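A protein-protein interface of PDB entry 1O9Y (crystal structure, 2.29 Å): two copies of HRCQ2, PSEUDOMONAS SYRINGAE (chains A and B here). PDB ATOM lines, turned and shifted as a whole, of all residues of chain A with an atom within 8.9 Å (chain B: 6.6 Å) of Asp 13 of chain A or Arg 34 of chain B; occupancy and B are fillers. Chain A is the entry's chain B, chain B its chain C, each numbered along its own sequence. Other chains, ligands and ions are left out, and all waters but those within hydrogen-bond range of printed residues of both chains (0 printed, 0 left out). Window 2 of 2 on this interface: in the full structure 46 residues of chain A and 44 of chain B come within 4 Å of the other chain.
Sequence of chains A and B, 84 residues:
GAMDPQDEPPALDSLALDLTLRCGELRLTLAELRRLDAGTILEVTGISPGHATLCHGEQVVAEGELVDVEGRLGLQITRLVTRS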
ATOM      1  N   ALA A  11      -2.761  -8.638   1.441  1.00  0.00           N
ATOM      2  CA  ALA A  11      -3.659  -9.511   0.634  1.00  0.00           C
ATOM      3  C   ALA A  11      -4.556  -8.642  -0.225  1.00  0.00           C
ATOM      4  O   ALA A  11      -5.314  -7.816   0.289  1.00  0.00           O
ATOM      5  CB  ALA A  11      -4.489 -10.410   1.529  1.00  0.00           C
ATOM      6  N   LEU A  12      -4.448  -8.842  -1.534  1.00  0.00           N
ATOM      7  CA  LEU A  12      -5.121  -8.039  -2.548  1.00  0.00           C
ATOM      8  C   LEU A  12      -4.706  -8.645  -3.883  1.00  0.00           C
ATOM      9  O   LEU A  12      -3.633  -9.259  -3.988  1.00  0.00           O
ATOM     10  CB  LEU A  12      -4.676  -6.562  -2.471  1.00  0.00           C
ATOM     11  CG  LEU A  12      -5.492  -5.357  -2.990  1.00  0.00           C
ATOM     12  CD1 LEU A  12      -6.994  -5.636  -3.229  1.00  0.00           C
ATOM     13  CD2 LEU A  12      -5.294  -4.152  -2.051  1.00  0.00           C
ATOM     14  N   ASP A  13      -5.545  -8.472  -4.900  1.00  0.00           N
ATOM     15  CA  ASP A  13      -5.258  -8.997  -6.232  1.00  0.00           C
ATOM     16  C   ASP A  13      -3.917  -8.506  -6.819  1.00  0.00           C
ATOM     17  O   ASP A  13      -3.343  -9.158  -7.691  1.00  0.00           O
ATOM     18  CB  ASP A  13      -6.440  -8.718  -7.180  1.00  0.00           C
ATOM     19  CG  ASP A  13      -7.525  -9.800  -7.105  1.00  0.00           C
ATOM     20  OD1 ASP A  13      -8.137 -10.122  -8.151  1.00  0.00           O
ATOM     21  OD2 ASP A  13      -7.836 -10.388  -6.045  1.00  0.00           O
ATOM     22  N   SER A  14      -3.415  -7.376  -6.320  1.00  0.00           N
ATOM     23  CA  SER A  14      -2.144  -6.803  -6.781  1.00  0.00           C
ATOM     24  C   SER A  14      -0.886  -7.444  -6.164  1.00  0.00           C
ATOM     25  O   SER A  14       0.240  -7.030  -6.471  1.00  0.00           O
ATOM     26  CB  SER A  14      -2.123  -5.283  -6.557  1.00  0.00           C
ATOM     27  N   LEU A  15      -1.073  -8.450  -5.310  1.00  0.00           N
ATOM     28  CA  LEU A  15       0.061  -9.130  -4.682  1.00  0.00           C
ATOM     29  C   LEU A  15       0.847  -9.955  -5.704  1.00  0.00           C
ATOM     30  O   LEU A  15       0.262 -10.750  -6.453  1.00  0.00           O
ATOM     31  CB  LEU A  15      -0.397 -10.002  -3.505  1.00  0.00           C
ATOM     32  CG  LEU A  15       0.709 -10.516  -2.578  1.00  0.00           C
ATOM     33  CD1 LEU A  15       1.150  -9.412  -1.626  1.00  0.00           C
ATOM     34  CD2 LEU A  15       0.238 -11.740  -1.814  1.00  0.00           C
ATOM     35  N   ALA A  16       2.165  -9.758  -5.715  1.00  0.00           N
ATOM     36  CA  ALA A  16       3.050 -10.326  -6.730  1.00  0.00           C
ATOM     37  C   ALA A  16       3.776 -11.571  -6.239  1.00  0.00           C
ATOM     38  O   ALA A  16       4.588 -11.507  -5.322  1.00  0.00           O
ATOM     39  CB  ALA A  16       4.058  -9.272  -7.204  1.00  0.00           C
ATOM     40  N   LEU A  17       3.483 -12.701  -6.867  1.00  0.00           N
ATOM     41  CA  LEU A  17       4.056 -13.981  -6.462  1.00  0.00           C
ATOM     42  C   LEU A  17       5.246 -14.365  -7.330  1.00  0.00           C
ATOM     43  O   LEU A  17       5.151 -14.370  -8.559  1.00  0.00           O
ATOM     44  CB  LEU A  17       2.993 -15.071  -6.530  1.00  0.00           C
ATOM     45  CG  LEU A  17       1.700 -14.826  -5.746  1.00  0.00           C
ATOM     46  CD1 LEU A  17       0.659 -15.792  -6.247  1.00  0.00           C
ATOM     47  CD2 LEU A  17       1.890 -14.973  -4.231  1.00  0.00           C
ATOM     48  N   LEU A  19       7.263 -17.142  -8.750  1.00  0.00           N
ATOM     49  CA  LEU A  19       6.994 -18.535  -9.043  1.00  0.00           C
ATOM     50  C   LEU A  19       8.196 -19.170  -9.724  1.00  0.00           C
ATOM     51  O   LEU A  19       8.993 -18.486 -10.359  1.00  0.00           O
ATOM     52  CB  LEU A  19       5.727 -18.685  -9.899  1.00  0.00           C
ATOM     53  CG  LEU A  19       4.423 -18.027  -9.427  1.00  0.00           C
ATOM     54  CD1 LEU A  19       3.429 -17.923 -10.556  1.00  0.00           C
ATOM     55  CD2 LEU A  19       3.789 -18.761  -8.265  1.00  0.00           C
ATOM     56  N   VAL A  61       0.862 -24.518  -8.244  1.00  0.00           N
ATOM     57  CA  VAL A  61      -0.290 -23.697  -8.607  1.00  0.00           C
ATOM     58  C   VAL A  61      -0.793 -23.994 -10.027  1.00  0.00           C
ATOM     59  O   VAL A  61      -1.940 -23.698 -10.351  1.00  0.00           O
ATOM     60  CB  VAL A  61      -0.042 -22.178  -8.405  1.00  0.00           C
ATOM     61  CG1 VAL A  61       0.322 -21.871  -6.941  1.00  0.00           C
ATOM     62  CG2 VAL A  61       1.028 -21.649  -9.347  1.00  0.00           C
ATOM     63  N   LEU A  80      -4.622 -25.747 -14.534  1.00  0.00           N
ATOM     64  CA  LEU A  80      -4.576 -24.898 -13.351  1.00  0.00           C
ATOM     65  C   LEU A  80      -4.929 -25.748 -12.124  1.00  0.00           C
ATOM     66  O   LEU A  80      -5.773 -26.644 -12.204  1.00  0.00           O
ATOM     67  CB  LEU A  80      -5.517 -23.700 -13.498  1.00  0.00           C
ATOM     68  CG  LEU A  80      -5.106 -22.442 -12.722  1.00  0.00           C
ATOM     69  N   THR B  29       0.967 -11.544 -10.426  1.00  0.00           N
ATOM     70  CA  THR B  29       0.072 -11.049  -9.385  1.00  0.00           C
ATOM     71  C   THR B  29      -1.002 -12.110  -9.089  1.00  0.00           C
ATOM     72  O   THR B  29      -1.235 -13.003  -9.907  1.00  0.00           O
ATOM     73  CB  THR B  29      -0.582  -9.701  -9.790  1.00  0.00           C
ATOM     74  OG1 THR B  29      -1.573  -9.931 -10.794  1.00  0.00           O
ATOM     75  CG2 THR B  29       0.415  -8.775 -10.478  1.00  0.00           C
ATOM     76  N   LEU B  30      -1.642 -12.007  -7.922  1.00  0.00           N
ATOM     77  CA  LEU B  30      -2.742 -12.893  -7.550  1.00  0.00           C
ATOM     78  C   LEU B  30      -3.880 -12.839  -8.583  1.00  0.00           C
ATOM     79  O   LEU B  30      -4.502 -13.855  -8.889  1.00  0.00           O
ATOM     80  CB  LEU B  30      -3.269 -12.524  -6.162  1.00  0.00           C
ATOM     81  CG  LEU B  30      -2.622 -13.240  -4.980  1.00  0.00           C
ATOM     82  N   ALA B  31      -4.130 -11.644  -9.113  1.00  0.00           N
ATOM     83  CA  ALA B  31      -5.153 -11.411 -10.133  1.00  0.00           C
ATOM     84  C   ALA B  31      -4.823 -12.146 -11.425  1.00  0.00           C
ATOM     85  O   ALA B  31      -5.691 -12.772 -12.022  1.00  0.00           O
ATOM     86  CB  ALA B  31      -5.314  -9.900 -10.400  1.00  0.00           C
ATOM     87  N   GLU B  32      -3.567 -12.070 -11.845  1.00  0.00           N
ATOM     88  CA  GLU B  32      -3.101 -12.767 -13.034  1.00  0.00           C
ATOM     89  C   GLU B  32      -3.206 -14.283 -12.885  1.00  0.00           C
ATOM     90  O   GLU B  32      -3.728 -14.961 -13.763  1.00  0.00           O
ATOM     91  CB  GLU B  32      -1.661 -12.371 -13.339  1.00  0.00           C
ATOM     92  CG  GLU B  32      -1.514 -10.981 -13.934  1.00  0.00           C
ATOM     93  CD  GLU B  32      -0.079 -10.493 -13.933  1.00  0.00           C
ATOM     94  OE1 GLU B  32       0.731 -11.022 -13.149  1.00  0.00           O
ATOM     95  OE2 GLU B  32       0.241  -9.576 -14.722  1.00  0.00           O
ATOM     96  N   LEU B  33      -2.717 -14.809 -11.765  1.00  0.00           N
ATOM     97  CA  LEU B  33      -2.752 -16.244 -11.511  1.00  0.00           C
ATOM     98  C   LEU B  33      -4.207 -16.735 -11.453  1.00  0.00           C
ATOM     99  O   LEU B  33      -4.507 -17.881 -11.819  1.00  0.00           O
ATOM    100  CB  LEU B  33      -1.983 -16.580 -10.222  1.00  0.00           C
ATOM    101  CG  LEU B  33      -2.006 -18.018  -9.692  1.00  0.00           C
ATOM    102  CD1 LEU B  33      -1.485 -19.028 -10.718  1.00  0.00           C
ATOM    103  CD2 LEU B  33      -1.214 -18.118  -8.403  1.00  0.00           C
ATOM    104  N   ARG B  34      -5.099 -15.847 -11.009  1.00  0.00           N
ATOM    105  CA  ARG B  34      -6.537 -16.107 -10.980  1.00  0.00           C
ATOM    106  C   ARG B  34      -7.106 -16.229 -12.392  1.00  0.00           C
ATOM    107  O   ARG B  34      -7.913 -17.124 -12.669  1.00  0.00           O
ATOM    108  CB  ARG B  34      -7.264 -15.000 -10.211  1.00  0.00           C
ATOM    109  CG  ARG B  34      -7.519 -15.341  -8.751  1.00  0.00           C
ATOM    110  CD  ARG B  34      -8.223 -14.247  -7.950  1.00  0.00           C
ATOM    111  NE  ARG B  34      -8.358 -14.610  -6.537  1.00  0.00           N
ATOM    112  CZ  ARG B  34      -7.502 -14.251  -5.583  1.00  0.00           C
ATOM    113  N   ARG B  35      -6.660 -15.334 -13.276  1.00  0.00           N
ATOM    114  CA  ARG B  35      -7.140 -15.247 -14.666  1.00  0.00           C
ATOM    115  C   ARG B  35      -6.608 -16.374 -15.548  1.00  0.00           C
ATOM    116  O   ARG B  35      -7.222 -16.732 -16.552  1.00  0.00           O
ATOM    117  CB  ARG B  35      -6.710 -13.913 -15.286  1.00  0.00           C
ATOM    118  CG  ARG B  35      -7.741 -12.797 -15.213  1.00  0.00           C
ATOM    119  CD  ARG B  35      -7.156 -11.383 -15.295  1.00  0.00           C
ATOM    120  NE  ARG B  35      -5.985 -11.298 -16.164  1.00  0.00           N
ATOM    121  N   LEU B  36      -5.458 -16.912 -15.162  1.00  0.00           N
ATOM    122  CA  LEU B  36      -4.697 -17.859 -15.962  1.00  0.00           C
ATOM    123  C   LEU B  36      -5.485 -19.116 -16.341  1.00  0.00           C
ATOM    124  O   LEU B  36      -5.886 -19.892 -15.475  1.00  0.00           O
ATOM    125  CB  LEU B  36      -3.428 -18.224 -15.196  1.00  0.00           C
ATOM    126  CG  LEU B  36      -2.385 -19.141 -15.822  1.00  0.00           C
ATOM    127  CD1 LEU B  36      -1.599 -18.401 -16.909  1.00  0.00           C
ATOM    128  CD2 LEU B  36      -1.463 -19.662 -14.727  1.00  0.00           C
ATOM    129  N   ASP B  37      -5.710 -19.304 -17.637  1.00  0.00           N
ATOM    130  CA  ASP B  37      -6.402 -20.493 -18.121  1.00  0.00           C
ATOM    131  C   ASP B  37      -5.467 -21.396 -18.923  1.00  0.00           C
ATOM    132  O   ASP B  37      -4.384 -20.966 -19.340  1.00  0.00           O
ATOM    133  CB  ASP B  37      -7.633 -20.109 -18.958  1.00  0.00           C
ATOM    134  CG  ASP B  37      -7.323 -19.061 -20.019  1.00  0.00           C
ATOM    135  OD1 ASP B  37      -6.373 -19.269 -20.812  1.00  0.00           O
ATOM    136  OD2 ASP B  37      -7.983 -17.998 -20.142  1.00  0.00           O
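O of Asp 13 of chain A is in hydrogen-bond range of N of Ala 31 of chain B, at 3.0 Å.
The backbone NH (N) of Leu 30 of chain B lies within hydrogen-bond range of the backbone carbonyl oxygen (O) of Leu 15 of chain A.
The backbone carbonyl oxygen (O) of Asp 13 of chain A is in hydrogen-bond range of the backbone NH (N) of Leu 30 of chain B (3.3 Å).
The backbone NH (N) of Thr 29 of chain B is in hydrogen-bond range of the side-chain carboxylate (OE1) of Glu 32 of chain B (2.8 Å).
Among the printed residues, merely in contact across the chains: Leu 12 of chain A with Leu 30 of chain B (3.9 Å), Asp 13 of chain A with Thr 29 of chain B (3.5 Å), Asp 13 of chain A with Arg 34 of chain B (3.9 Å), Leu 15 of chain A with Thr 29 of chain B (3.0 Å), Leu 17 of chain A with Leu 33 of chain B (3.7 Å), Val 61 of chain A with Leu 33 of chain B (3.9 Å) and Leu 80 of chain A with Leu 36 of chain B (3.8 Å).
Of the printed residues of chain B, Leu 12 of chain A touches Leu 30 (3.9 Å).
Of chain B, only Thr 29, Leu 30, Ala 31 and Arg 34 come within 4 Å of Asp 13 of chain A.
Printed residues of chain A within 4 Å of Thr 29 of chain B: Asp 13 (3.5 Å) and Leu 15 (3.0 Å).
Printed residues of chain A within 4 Å of Leu 30 of chain B: Leu 12 (3.9 Å), Asp 13 (3.3 Å) and Leu 15 (2.7 Å).
Ala 31 of chain B touches one residue of chain A.
Printed residues of chain A within 4 Å of Leu 33 of chain B: Leu 17 and Val 61.
Of chain A, only Asp 13 comes within 4 Å of Arg 34 of chain B.
The nearest residue of chain B that does not touch Asp 13 of chain A is Glu 32 of chain B (5.1 Å).
The nearest residue of chain A that does not touch Arg 34 of chain B is Leu 80 of chain A (6.0 Å).
The nearest printed residue of chain A that does not touch Leu 33 of chain B is Leu 80 of chain A (4.7 Å).
Of the 10 printed residues of chain A, 6 touch a printed residue of chain B.
Hydrophobic or aromatic side chains of chain A within 4 Å of the printed part of chain B: Leu 17, Val 61 and Leu 80.
Hydrophobic or aromatic side chains of chain B that line the printed part of chain A: Leu 30, Ala 31 and Leu 33.
Among the printed residues, 10 pairs touch across the chains.
Among the printed residues, no Asp or Glu carboxylate lies within 4 Å of a Lys or Arg side-chain nitrogen of the other chain.
No position is printed for both chains.
Of the 10 pairs that touch across the chains among the printed residues, none has its exchanged pair printed and touching as well.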
